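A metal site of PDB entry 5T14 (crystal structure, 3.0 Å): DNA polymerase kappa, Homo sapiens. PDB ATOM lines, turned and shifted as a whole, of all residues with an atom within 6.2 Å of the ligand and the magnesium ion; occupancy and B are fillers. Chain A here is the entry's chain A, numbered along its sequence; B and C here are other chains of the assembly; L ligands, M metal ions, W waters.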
ATOM      1  N   ASP A 107       7.485 -24.456   2.190  1.00  0.00           N
ATOM      2  CA  ASP A 107       7.355 -23.009   2.367  1.00  0.00           C
ATOM      3  C   ASP A 107       8.499 -22.367   1.606  1.00  0.00           C
ATOM      4  O   ASP A 107       9.658 -22.576   1.956  1.00  0.00           O
ATOM      5  CB  ASP A 107       7.424 -22.663   3.860  1.00  0.00           C
ATOM      6  CG  ASP A 107       7.070 -21.218   4.157  1.00  0.00           C
ATOM      7  OD1 ASP A 107       7.375 -20.314   3.349  1.00  0.00           O
ATOM      8  OD2 ASP A 107       6.490 -20.970   5.245  1.00  0.00           O
ATOM      9  N   MET A 108       8.180 -21.581   0.576  1.00  0.00           N
ATOM     10  CA  MET A 108       9.229 -20.885  -0.178  1.00  0.00           C
ATOM     11  C   MET A 108       9.895 -19.800   0.674  1.00  0.00           C
ATOM     12  O   MET A 108       9.263 -19.180   1.555  1.00  0.00           O
ATOM     13  CB  MET A 108       8.673 -20.253  -1.454  1.00  0.00           C
ATOM     14  CG  MET A 108       8.092 -21.249  -2.432  1.00  0.00           C
ATOM     15  SD  MET A 108       9.350 -22.083  -3.399  1.00  0.00           S
ATOM     16  CE  MET A 108       8.622 -23.711  -3.397  1.00  0.00           C
ATOM     17  N   ASP A 109      11.192 -19.594   0.391  1.00  0.00           N
ATOM     18  CA  ASP A 109      12.020 -18.624   1.087  1.00  0.00           C
ATOM     19  C   ASP A 109      11.886 -17.277   0.408  1.00  0.00           C
ATOM     20  O   ASP A 109      11.978 -17.199  -0.812  1.00  0.00           O
ATOM     21  CB  ASP A 109      13.488 -19.050   1.060  1.00  0.00           C
ATOM     22  CG  ASP A 109      13.725 -20.444   1.636  1.00  0.00           C
ATOM     23  OD1 ASP A 109      13.055 -20.815   2.638  1.00  0.00           O
ATOM     24  OD2 ASP A 109      14.599 -21.158   1.094  1.00  0.00           O
ATOM     25  N   ALA A 110      11.678 -16.237   1.196  1.00  0.00           N
ATOM     26  CA  ALA A 110      11.583 -14.864   0.698  1.00  0.00           C
ATOM     27  C   ALA A 110      10.894 -14.767  -0.677  1.00  0.00           C
ATOM     28  O   ALA A 110      11.420 -14.141  -1.596  1.00  0.00           O
ATOM     29  CB  ALA A 110      12.973 -14.251   0.645  1.00  0.00           C
ATOM     30  N   PHE A 111       9.716 -15.375  -0.789  1.00  0.00           N
ATOM     31  CA  PHE A 111       9.170 -15.772  -2.099  1.00  0.00           C
ATOM     32  C   PHE A 111       9.167 -14.686  -3.177  1.00  0.00           C
ATOM     33  O   PHE A 111       9.905 -14.801  -4.155  1.00  0.00           O
ATOM     34  CB  PHE A 111       7.782 -16.406  -1.939  1.00  0.00           C
ATOM     35  CG  PHE A 111       7.199 -16.945  -3.224  1.00  0.00           C
ATOM     36  CD1 PHE A 111       7.925 -17.835  -4.007  1.00  0.00           C
ATOM     37  CD2 PHE A 111       5.921 -16.584  -3.622  1.00  0.00           C
ATOM     38  CE1 PHE A 111       7.385 -18.330  -5.188  1.00  0.00           C
ATOM     39  CE2 PHE A 111       5.380 -17.079  -4.802  1.00  0.00           C
ATOM     40  CZ  PHE A 111       6.113 -17.963  -5.582  1.00  0.00           C
ATOM     41  N   TYR A 112       8.377 -13.630  -2.989  1.00  0.00           N
ATOM     42  CA  TYR A 112       8.294 -12.603  -4.020  1.00  0.00           C
ATOM     43  C   TYR A 112       9.673 -11.985  -4.256  1.00  0.00           C
ATOM     44  O   TYR A 112      10.026 -11.687  -5.393  1.00  0.00           O
ATOM     45  CB  TYR A 112       7.258 -11.506  -3.688  1.00  0.00           C
ATOM     46  CG  TYR A 112       5.788 -11.908  -3.571  1.00  0.00           C
ATOM     47  CD1 TYR A 112       5.346 -13.209  -3.830  1.00  0.00           C
ATOM     48  CD2 TYR A 112       4.821 -10.961  -3.240  1.00  0.00           C
ATOM     49  CE1 TYR A 112       4.009 -13.554  -3.711  1.00  0.00           C
ATOM     50  CE2 TYR A 112       3.479 -11.299  -3.126  1.00  0.00           C
ATOM     51  CZ  TYR A 112       3.071 -12.602  -3.361  1.00  0.00           C
ATOM     52  OH  TYR A 112       1.736 -12.934  -3.245  1.00  0.00           O
ATOM     53  N   ALA A 113      10.467 -11.818  -3.188  1.00  0.00           N
ATOM     54  CA  ALA A 113      11.838 -11.278  -3.272  1.00  0.00           C
ATOM     55  C   ALA A 113      12.808 -12.184  -4.021  1.00  0.00           C
ATOM     56  O   ALA A 113      13.540 -11.725  -4.892  1.00  0.00           O
ATOM     57  CB  ALA A 113      12.370 -10.998  -1.880  1.00  0.00           C
ATOM     58  N   MET A 135       3.561   0.141   1.064  1.00  0.00           N
ATOM     59  CA  MET A 135       3.508  -1.168   1.729  1.00  0.00           C
ATOM     60  C   MET A 135       4.473  -2.168   1.125  1.00  0.00           C
ATOM     61  O   MET A 135       4.723  -2.159  -0.081  1.00  0.00           O
ATOM     62  CB  MET A 135       2.077  -1.720   1.652  1.00  0.00           C
ATOM     63  CG  MET A 135       1.797  -2.949   2.500  1.00  0.00           C
ATOM     64  SD  MET A 135       2.147  -2.738   4.257  1.00  0.00           S
ATOM     65  CE  MET A 135       1.076  -1.374   4.693  1.00  0.00           C
ATOM     66  N   LEU A 136       5.010  -3.045   1.981  1.00  0.00           N
ATOM     67  CA  LEU A 136       5.904  -4.116   1.558  1.00  0.00           C
ATOM     68  C   LEU A 136       5.282  -5.500   1.817  1.00  0.00           C
ATOM     69  O   LEU A 136       4.972  -5.857   2.950  1.00  0.00           O
ATOM     70  CB  LEU A 136       7.247  -3.998   2.295  1.00  0.00           C
ATOM     71  CG  LEU A 136       8.011  -2.670   2.222  1.00  0.00           C
ATOM     72  CD1 LEU A 136       9.366  -2.819   2.876  1.00  0.00           C
ATOM     73  CD2 LEU A 136       8.200  -2.167   0.795  1.00  0.00           C
ATOM     74  N   SER A 137       5.088  -6.265   0.744  1.00  0.00           N
ATOM     75  CA  SER A 137       4.655  -7.644   0.859  1.00  0.00           C
ATOM     76  C   SER A 137       5.696  -8.457   1.608  1.00  0.00           C
ATOM     77  O   SER A 137       5.366  -9.165   2.547  1.00  0.00           O
ATOM     78  CB  SER A 137       4.465  -8.251  -0.525  1.00  0.00           C
ATOM     79  OG  SER A 137       3.469  -7.544  -1.252  1.00  0.00           O
ATOM     80  N   THR A 138       6.943  -8.368   1.160  1.00  0.00           N
ATOM     81  CA  THR A 138       8.035  -9.094   1.773  1.00  0.00           C
ATOM     82  C   THR A 138       9.369  -8.432   1.483  1.00  0.00           C
ATOM     83  O   THR A 138       9.445  -7.492   0.695  1.00  0.00           O
ATOM     84  CB  THR A 138       8.083 -10.544   1.268  1.00  0.00           C
ATOM     85  OG1 THR A 138       9.003 -11.309   2.059  1.00  0.00           O
ATOM     86  CG2 THR A 138       8.496 -10.610  -0.216  1.00  0.00           C
ATOM     87  N   SER A 139      10.398  -8.977   2.117  1.00  0.00           N
ATOM     88  CA  SER A 139      11.783  -8.560   1.901  1.00  0.00           C
ATOM     89  C   SER A 139      12.695  -9.754   1.956  1.00  0.00           C
ATOM     90  O   SER A 139      12.381 -10.750   2.620  1.00  0.00           O
ATOM     91  CB  SER A 139      12.190  -7.619   2.998  1.00  0.00           C
ATOM     92  OG  SER A 139      12.141  -8.295   4.243  1.00  0.00           O
ATOM     93  N   TYR A 141      16.409 -11.742   2.855  1.00  0.00           N
ATOM     94  CA  TYR A 141      17.128 -11.911   4.120  1.00  0.00           C
ATOM     95  C   TYR A 141      18.211 -10.862   4.363  1.00  0.00           C
ATOM     96  O   TYR A 141      18.430 -10.468   5.511  1.00  0.00           O
ATOM     97  CB  TYR A 141      17.671 -13.337   4.232  1.00  0.00           C
ATOM     98  CG  TYR A 141      16.567 -14.328   4.530  1.00  0.00           C
ATOM     99  CD1 TYR A 141      15.828 -14.918   3.511  1.00  0.00           C
ATOM    100  CD2 TYR A 141      16.213 -14.630   5.841  1.00  0.00           C
ATOM    101  CE1 TYR A 141      14.805 -15.816   3.790  1.00  0.00           C
ATOM    102  CE2 TYR A 141      15.191 -15.520   6.131  1.00  0.00           C
ATOM    103  CZ  TYR A 141      14.494 -16.104   5.102  1.00  0.00           C
ATOM    104  OH  TYR A 141      13.493 -16.975   5.402  1.00  0.00           O
ATOM    105  N   ARG A 144      16.336  -8.006   5.793  1.00  0.00           N
ATOM    106  CA  ARG A 144      15.789  -8.308   7.121  1.00  0.00           C
ATOM    107  C   ARG A 144      16.749  -8.031   8.298  1.00  0.00           C
ATOM    108  O   ARG A 144      16.295  -7.729   9.408  1.00  0.00           O
ATOM    109  CB  ARG A 144      15.286  -9.756   7.180  1.00  0.00           C
ATOM    110  CG  ARG A 144      13.973  -9.934   6.467  1.00  0.00           C
ATOM    111  CD  ARG A 144      13.452 -11.351   6.568  1.00  0.00           C
ATOM    112  NE  ARG A 144      12.543 -11.640   5.466  1.00  0.00           N
ATOM    113  CZ  ARG A 144      11.920 -12.798   5.281  1.00  0.00           C
ATOM    114  NH1 ARG A 144      12.095 -13.808   6.135  1.00  0.00           N
ATOM    115  NH2 ARG A 144      11.124 -12.945   4.243  1.00  0.00           N
ATOM    116  N   ALA A 150       7.824  -7.893   6.072  1.00  0.00           N
ATOM    117  CA  ALA A 150       6.448  -7.956   5.583  1.00  0.00           C
ATOM    118  C   ALA A 150       5.516  -7.072   6.425  1.00  0.00           C
ATOM    119  O   ALA A 150       5.630  -7.043   7.634  1.00  0.00           O
ATOM    120  CB  ALA A 150       5.958  -9.398   5.600  1.00  0.00           C
ATOM    121  N   ALA A 151       4.622  -6.355   5.739  1.00  0.00           N
ATOM    122  CA  ALA A 151       3.613  -5.478   6.344  1.00  0.00           C
ATOM    123  C   ALA A 151       4.139  -4.124   6.821  1.00  0.00           C
ATOM    124  O   ALA A 151       3.346  -3.321   7.321  1.00  0.00           O
ATOM    125  CB  ALA A 151       2.846  -6.171   7.463  1.00  0.00           C
ATOM    126  N   SER A 196      -1.471 -21.352   0.035  1.00  0.00           N
ATOM    127  CA  SER A 196      -1.144 -20.052  -0.515  1.00  0.00           C
ATOM    128  C   SER A 196      -0.419 -20.310  -1.848  1.00  0.00           C
ATOM    129  O   SER A 196      -0.414 -21.440  -2.342  1.00  0.00           O
ATOM    130  CB  SER A 196      -0.266 -19.300   0.495  1.00  0.00           C
ATOM    131  OG  SER A 196       0.745 -18.511  -0.111  1.00  0.00           O
ATOM    132  N   ASP A 198       2.971 -19.720  -2.066  1.00  0.00           N
ATOM    133  CA  ASP A 198       4.289 -20.191  -1.626  1.00  0.00           C
ATOM    134  C   ASP A 198       4.278 -21.359  -0.635  1.00  0.00           C
ATOM    135  O   ASP A 198       5.351 -21.859  -0.292  1.00  0.00           O
ATOM    136  CB  ASP A 198       5.107 -19.017  -1.040  1.00  0.00           C
ATOM    137  CG  ASP A 198       4.998 -18.882   0.486  1.00  0.00           C
ATOM    138  OD1 ASP A 198       3.850 -18.772   0.974  1.00  0.00           O
ATOM    139  OD2 ASP A 198       6.042 -18.870   1.183  1.00  0.00           O
ATOM    140  N   GLU A 199       3.106 -21.790  -0.157  1.00  0.00           N
ATOM    141  CA  GLU A 199       3.015 -22.812   0.902  1.00  0.00           C
ATOM    142  C   GLU A 199       2.053 -23.938   0.576  1.00  0.00           C
ATOM    143  O   GLU A 199       1.161 -23.786  -0.258  1.00  0.00           O
ATOM    144  CB  GLU A 199       2.622 -22.155   2.233  1.00  0.00           C
ATOM    145  CG  GLU A 199       3.810 -21.480   2.930  1.00  0.00           C
ATOM    146  CD  GLU A 199       3.419 -20.547   4.066  1.00  0.00           C
ATOM    147  OE1 GLU A 199       2.908 -21.048   5.112  1.00  0.00           O
ATOM    148  OE2 GLU A 199       3.673 -19.320   3.932  1.00  0.00           O
ATOM    149  N   ASP A 325       9.599 -23.596   9.775  1.00  0.00           N
ATOM    150  CA  ASP A 325      10.256 -22.337  10.154  1.00  0.00           C
ATOM    151  C   ASP A 325      11.639 -22.567  10.787  1.00  0.00           C
ATOM    152  O   ASP A 325      12.526 -21.711  10.648  1.00  0.00           O
ATOM    153  CB  ASP A 325       9.352 -21.557  11.117  1.00  0.00           C
ATOM    154  CG  ASP A 325       9.885 -20.169  11.441  1.00  0.00           C
ATOM    155  OD1 ASP A 325      10.205 -19.417  10.496  1.00  0.00           O
ATOM    156  OD2 ASP A 325       9.966 -19.823  12.644  1.00  0.00           O
ATOM    157  N   LYS A 328      15.023 -22.377   8.365  1.00  0.00           N
ATOM    158  CA  LYS A 328      14.808 -21.504   7.209  1.00  0.00           C
ATOM    159  C   LYS A 328      15.926 -20.461   7.193  1.00  0.00           C
ATOM    160  O   LYS A 328      16.295 -19.975   8.259  1.00  0.00           O
ATOM    161  CB  LYS A 328      13.443 -20.821   7.338  1.00  0.00           C
ATOM    162  CG  LYS A 328      12.955 -20.070   6.115  1.00  0.00           C
ATOM    163  CD  LYS A 328      11.576 -19.435   6.346  1.00  0.00           C
ATOM    164  CE  LYS A 328      10.439 -20.252   5.734  1.00  0.00           C
ATOM    165  NZ  LYS A 328      10.381 -20.135   4.252  1.00  0.00           N
ATOM    166  N   PRO A 329      16.481 -20.078   6.035  1.00  0.00           N
ATOM    167  CA  PRO A 329      16.091 -20.555   4.704  1.00  0.00           C
ATOM    168  C   PRO A 329      16.828 -21.784   4.252  1.00  0.00           C
ATOM    169  O   PRO A 329      17.885 -22.103   4.772  1.00  0.00           O
ATOM    170  CB  PRO A 329      16.503 -19.403   3.780  1.00  0.00           C
ATOM    171  CG  PRO A 329      17.459 -18.580   4.564  1.00  0.00           C
ATOM    172  CD  PRO A 329      17.023 -18.708   5.985  1.00  0.00           C
ATOM    173  P    DT B   4      -2.862   0.319   5.056  1.00  0.00           P
ATOM    174  OP1  DT B   4      -3.657   1.473   4.558  1.00  0.00           O
ATOM    175  OP2  DT B   4      -3.392  -0.560   6.125  1.00  0.00           O
ATOM    176  O5'  DT B   4      -2.501  -0.589   3.805  1.00  0.00           O
ATOM    177  C5'  DT B   4      -2.017  -0.007   2.584  1.00  0.00           C
ATOM    178  C4'  DT B   4      -2.262  -0.961   1.440  1.00  0.00           C
ATOM    179  O4'  DT B   4      -1.460  -2.146   1.628  1.00  0.00           O
ATOM    180  C3'  DT B   4      -3.706  -1.451   1.325  1.00  0.00           C
ATOM    181  O3'  DT B   4      -4.079  -1.554  -0.054  1.00  0.00           O
ATOM    182  C2'  DT B   4      -3.678  -2.799   2.019  1.00  0.00           C
ATOM    183  C1'  DT B   4      -2.282  -3.301   1.728  1.00  0.00           C
ATOM    184  N1   DT B   4      -1.693  -4.185   2.745  1.00  0.00           N
ATOM    185  C2   DT B   4      -1.162  -5.386   2.343  1.00  0.00           C
ATOM    186  O2   DT B   4      -1.173  -5.767   1.184  1.00  0.00           O
ATOM    187  N3   DT B   4      -0.616  -6.142   3.347  1.00  0.00           N
ATOM    188  C4   DT B   4      -0.550  -5.816   4.694  1.00  0.00           C
ATOM    189  O4   DT B   4      -0.019  -6.593   5.483  1.00  0.00           O
ATOM    190  C5   DT B   4      -1.127  -4.543   5.045  1.00  0.00           C
ATOM    191  C7   DT B   4      -1.101  -4.105   6.472  1.00  0.00           C
ATOM    192  C6   DT B   4      -1.651  -3.793   4.070  1.00  0.00           C
ATOM    193  O1  VKJ B   5      -2.802  -8.325   4.939  1.00  0.00           O
ATOM    194  C1  VKJ B   5      -3.412  -8.509   3.877  1.00  0.00           C
ATOM    195  N1  VKJ B   5      -3.421  -9.815   3.395  1.00  0.00           N
ATOM    196  C2  VKJ B   5      -4.084 -10.176   2.243  1.00  0.00           C
ATOM    197  N2  VKJ B   5      -3.956 -11.470   1.913  1.00  0.00           N
ATOM    198  N3  VKJ B   5      -4.767  -9.325   1.481  1.00  0.00           N
ATOM    199  C3  VKJ B   5      -4.730  -8.056   1.943  1.00  0.00           C
ATOM    200  C4  VKJ B   5      -4.122  -7.579   3.075  1.00  0.00           C
ATOM    201  N4  VKJ B   5      -4.351  -6.228   3.223  1.00  0.00           N
ATOM    202  C5  VKJ B   5      -5.066  -5.905   2.179  1.00  0.00           C
ATOM    203  N5  VKJ B   5      -5.376  -6.992   1.397  1.00  0.00           N
ATOM    204  C6  VKJ B   5      -6.012  -6.958   0.099  1.00  0.00           C
ATOM    205  O2  VKJ B   5      -5.023  -6.329  -0.739  1.00  0.00           O
ATOM    206  C7  VKJ B   5      -7.247  -6.103  -0.136  1.00  0.00           C
ATOM    207  C8  VKJ B   5      -7.131  -5.858  -1.632  1.00  0.00           C
ATOM    208  O3  VKJ B   5      -7.460  -7.054  -2.337  1.00  0.00           O
ATOM    209  C9  VKJ B   5      -5.635  -5.617  -1.826  1.00  0.00           C
ATOM    210  C10 VKJ B   5      -5.219  -4.165  -1.860  1.00  0.00           C
ATOM    211  O4  VKJ B   5      -5.562  -3.522  -0.614  1.00  0.00           O
ATOM    212  P1  VKJ B   5      -5.595  -1.921  -0.460  1.00  0.00           P
ATOM    213  O5  VKJ B   5      -6.481  -1.613   0.675  1.00  0.00           O
ATOM    214  O6  VKJ B   5      -5.862  -1.278  -1.764  1.00  0.00           O
ATOM    215  O7  VKJ B   5      -6.028 -14.008   0.345  1.00  0.00           O
ATOM    216  C11 VKJ B   5      -5.039 -13.464   1.249  1.00  0.00           C
ATOM    217  C12 VKJ B   5      -4.607 -12.093   0.765  1.00  0.00           C
ATOM    218  C13 VKJ B   5      -3.667 -12.229  -0.465  1.00  0.00           C
ATOM    219  C14 VKJ B   5      -3.875 -14.417   1.426  1.00  0.00           C
ATOM    220  O8  VKJ B   5      -4.310 -15.568   2.172  1.00  0.00           O
ATOM    221  C15 VKJ B   5      -3.335 -14.803   0.037  1.00  0.00           C
ATOM    222  O9  VKJ B   5      -1.983 -15.320   0.141  1.00  0.00           O
ATOM    223  C16 VKJ B   5      -3.390 -13.645  -0.910  1.00  0.00           C
ATOM    224  C17 VKJ B   5      -2.969 -13.967  -2.198  1.00  0.00           C
ATOM    225  C18 VKJ B   5      -2.909 -13.060  -3.236  1.00  0.00           C
ATOM    226  C19 VKJ B   5      -3.285 -11.675  -2.925  1.00  0.00           C
ATOM    227  C20 VKJ B   5      -3.755 -11.264  -1.583  1.00  0.00           C
ATOM    228  C21 VKJ B   5      -4.037  -9.910  -1.422  1.00  0.00           C
ATOM    229  C22 VKJ B   5      -3.977  -9.006  -2.485  1.00  0.00           C
ATOM    230  C23 VKJ B   5      -3.219 -10.699  -4.027  1.00  0.00           C
ATOM    231  C24 VKJ B   5      -2.802 -11.118  -5.293  1.00  0.00           C
ATOM    232  C25 VKJ B   5      -2.454 -12.460  -5.535  1.00  0.00           C
ATOM    233  C26 VKJ B   5      -2.499 -13.417  -4.523  1.00  0.00           C
ATOM    234  C27 VKJ B   5      -2.759 -10.170  -6.316  1.00  0.00           C
ATOM    235  C28 VKJ B   5      -3.582  -9.381  -3.765  1.00  0.00           C
ATOM    236  C29 VKJ B   5      -3.529  -8.442  -4.791  1.00  0.00           C
ATOM    237  C30 VKJ B   5      -3.119  -8.833  -6.069  1.00  0.00           C
ATOM    238  P    DC C   9       1.484 -17.812   7.419  1.00  0.00           P
ATOM    239  OP1  DC C   9       2.134 -19.101   7.097  1.00  0.00           O
ATOM    240  OP2  DC C   9       2.210 -16.754   8.196  1.00  0.00           O
ATOM    241  O5'  DC C   9       1.007 -17.133   6.061  1.00  0.00           O
ATOM    242  C5'  DC C   9      -0.079 -17.693   5.281  1.00  0.00           C
ATOM    243  C4'  DC C   9      -0.074 -17.102   3.892  1.00  0.00           C
ATOM    244  O4'  DC C   9      -0.768 -15.835   3.904  1.00  0.00           O
ATOM    245  C3'  DC C   9       1.312 -16.823   3.315  1.00  0.00           C
ATOM    246  O3'  DC C   9       1.352 -17.081   1.912  1.00  0.00           O
ATOM    247  C2'  DC C   9       1.504 -15.342   3.567  1.00  0.00           C
ATOM    248  C1'  DC C   9       0.097 -14.804   3.445  1.00  0.00           C
ATOM    249  N1   DC C   9      -0.199 -13.595   4.240  1.00  0.00           N
ATOM    250  C2   DC C   9      -0.969 -12.572   3.670  1.00  0.00           C
ATOM    251  O2   DC C   9      -1.335 -12.699   2.488  1.00  0.00           O
ATOM    252  N3   DC C   9      -1.249 -11.471   4.393  1.00  0.00           N
ATOM    253  C4   DC C   9      -0.818 -11.373   5.652  1.00  0.00           C
ATOM    254  N4   DC C   9      -1.114 -10.267   6.338  1.00  0.00           N
ATOM    255  C5   DC C   9      -0.037 -12.399   6.268  1.00  0.00           C
ATOM    256  C6   DC C   9       0.234 -13.486   5.535  1.00  0.00           C
HETATM  257  N1  LIG L   1       0.875  -8.534   2.822  1.00  0.00           N
HETATM  258  C1  LIG L   1       0.991  -8.897   1.534  1.00  0.00           C
HETATM  259  N2  LIG L   1       1.686  -9.931   1.027  1.00  0.00           N
HETATM  260  C2  LIG L   1       2.319 -10.627   2.000  1.00  0.00           C
HETATM  261  C3  LIG L   1       2.280 -10.362   3.354  1.00  0.00           C
HETATM  262  C4  LIG L   1       1.527  -9.258   3.778  1.00  0.00           C
HETATM  263  N3  LIG L   1       1.428  -8.903   5.079  1.00  0.00           N
HETATM  264  N4  LIG L   1       3.048 -11.297   4.035  1.00  0.00           N
HETATM  265  C5  LIG L   1       3.505 -12.083   3.092  1.00  0.00           C
HETATM  266  N5  LIG L   1       3.086 -11.744   1.862  1.00  0.00           N
HETATM  267  P1  LIG L   1       5.667 -15.697   3.715  1.00  0.00           P
HETATM  268  P2  LIG L   1       8.297 -15.035   2.662  1.00  0.00           P
HETATM  269  P3  LIG L   1       9.931 -16.507   4.496  1.00  0.00           P
HETATM  270  C6  LIG L   1       3.452 -12.390   0.571  1.00  0.00           C
HETATM  271  O1  LIG L   1       6.009 -17.108   3.536  1.00  0.00           O
HETATM  272  O2  LIG L   1       8.129 -16.284   1.932  1.00  0.00           O
HETATM  273  O3  LIG L   1      11.294 -16.934   4.026  1.00  0.00           O
HETATM  274  C7  LIG L   1       4.892 -12.060   0.217  1.00  0.00           C
HETATM  275  O4  LIG L   1       4.970 -15.409   5.083  1.00  0.00           O
HETATM  276  O5  LIG L   1       8.497 -13.795   1.644  1.00  0.00           O
HETATM  277  O6  LIG L   1       9.801 -16.026   5.929  1.00  0.00           O
HETATM  278  C8  LIG L   1       5.645 -13.361   0.402  1.00  0.00           C
HETATM  279  O7  LIG L   1       6.654 -13.535  -0.610  1.00  0.00           O
HETATM  280  N6  LIG L   1       7.009 -14.783   3.624  1.00  0.00           N
HETATM  281  O8  LIG L   1       9.586 -15.228   3.592  1.00  0.00           O
HETATM  282  O9  LIG L   1       8.810 -17.500   4.250  1.00  0.00           O
HETATM  283  C9  LIG L   1       4.568 -14.435   0.294  1.00  0.00           C
HETATM  284  O10 LIG L   1       3.341 -13.805   0.679  1.00  0.00           O
HETATM  285  C10 LIG L   1       4.830 -15.621   1.191  1.00  0.00           C
HETATM  286  O11 LIG L   1       4.667 -15.225   2.550  1.00  0.00           O
HETATM  287 MG    MG M   1       7.583 -18.279   2.625  1.00  0.00          MG
HETATM  288  O   HOH W   1       2.683 -10.762   7.288  1.00  0.00           O
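OG1 of Thr 138 is in hydrogen-bond range of O5 of the ligand (2.6 Å). O3 of the ligand sits at hydrogen-bond distance from OH of Tyr 141 (2.6 Å). O4 of DT 4 of chain B lies within hydrogen-bond range of a nitrogen (N3) of the ligand. The guanidinium group (NH1) of Arg 144 lies within salt-bridge range of an oxygen (O6) of the ligand (3.2 Å). The backbone NH of Tyr 112 sits at hydrogen-bond distance from an oxygen (O7) of the ligand. The backbone NH (N) of Ala 110 sits at hydrogen-bond distance from an oxygen (O3) of the ligand (2.9 Å). NZ of Lys 328 lies within salt-bridge range of O3 of the ligand (3.3 Å). N of Phe 111 is in hydrogen-bond range of O5 of the ligand, 3.1 Å away. N4 of DC 9 of chain C is in hydrogen-bond range of a nitrogen (N3) of the ligand (3.1 Å).
The side-chain amino group (NZ) of Lys 328 sits at hydrogen-bond distance from the backbone carbonyl oxygen (O) of Asp 107 (3.4 Å). The backbone carbonyl oxygen (O) of Met 108 sits close to the side-chain amino group (NZ) of Lys 328 (3.1 Å). The guanidinium group (NH2) of Arg 144 sits at hydrogen-bond distance from the side-chain hydroxyl (OG1) of Thr 138. The backbone carbonyl oxygen of Ser 139 is in hydrogen-bond range of the guanidinium group of Arg 144 (3.0 Å). The side-chain amino group (NZ) of Lys 328 lies within salt-bridge range of the side-chain carboxylate (OD1) of Asp 109 (3.2 Å). N1 of VKJ 5 of chain B lies within hydrogen-bond range of N3 of DC 9 of chain C (2.9 Å). The side-chain hydroxyl of Ser 196 is in hydrogen-bond range of O3' of DC 9 of chain C. The backbone NH (N) of Ala 151 sits at hydrogen-bond distance from the backbone carbonyl oxygen (O) of Leu 136 (2.9 Å).
The backbone carbonyl oxygen (O) of Ser 137 lies close to a nitrogen (N4) of the ligand, at 3.5 Å. O1 of the ligand sits close to OE2 of Glu 199 (3.2 Å). Merely in contact with the ligand: Asp 109 (3.5 Å), Ala 150 (3.8 Å) and Ala 151 (3.9 Å). Hydrophobic or aromatic side chains within 4 Å of the ligand: Phe 111, Tyr 112, Tyr 141, Ala 150 and Ala 151.
Residues that only touch the magnesium ion: Lys 328. Within 4 Å of the magnesium ion: Asp 107, Met 108, Asp 198 and Lys 328. Along chain A the residues within 4 Å of the magnesium ion span positions 107 to 328. The nearest printed residue that does not touch the magnesium ion is Glu 199 (4.3 Å).
The magnesium ion is bound by an oxygen (O1) of the ligand (2.2 Å), the side-chain carboxylate (OD1) of Asp 107 (2.2 Å), an oxygen (O9) of the ligand (2.2 Å), an oxygen (O2) of the ligand (2.2 Å), the backbone carbonyl oxygen (O) of Met 108 (2.2 Å) and the side-chain carboxylate (OD2) of Asp 198 (2.2 Å). The magnesium ion has six donor atoms within binding distance.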
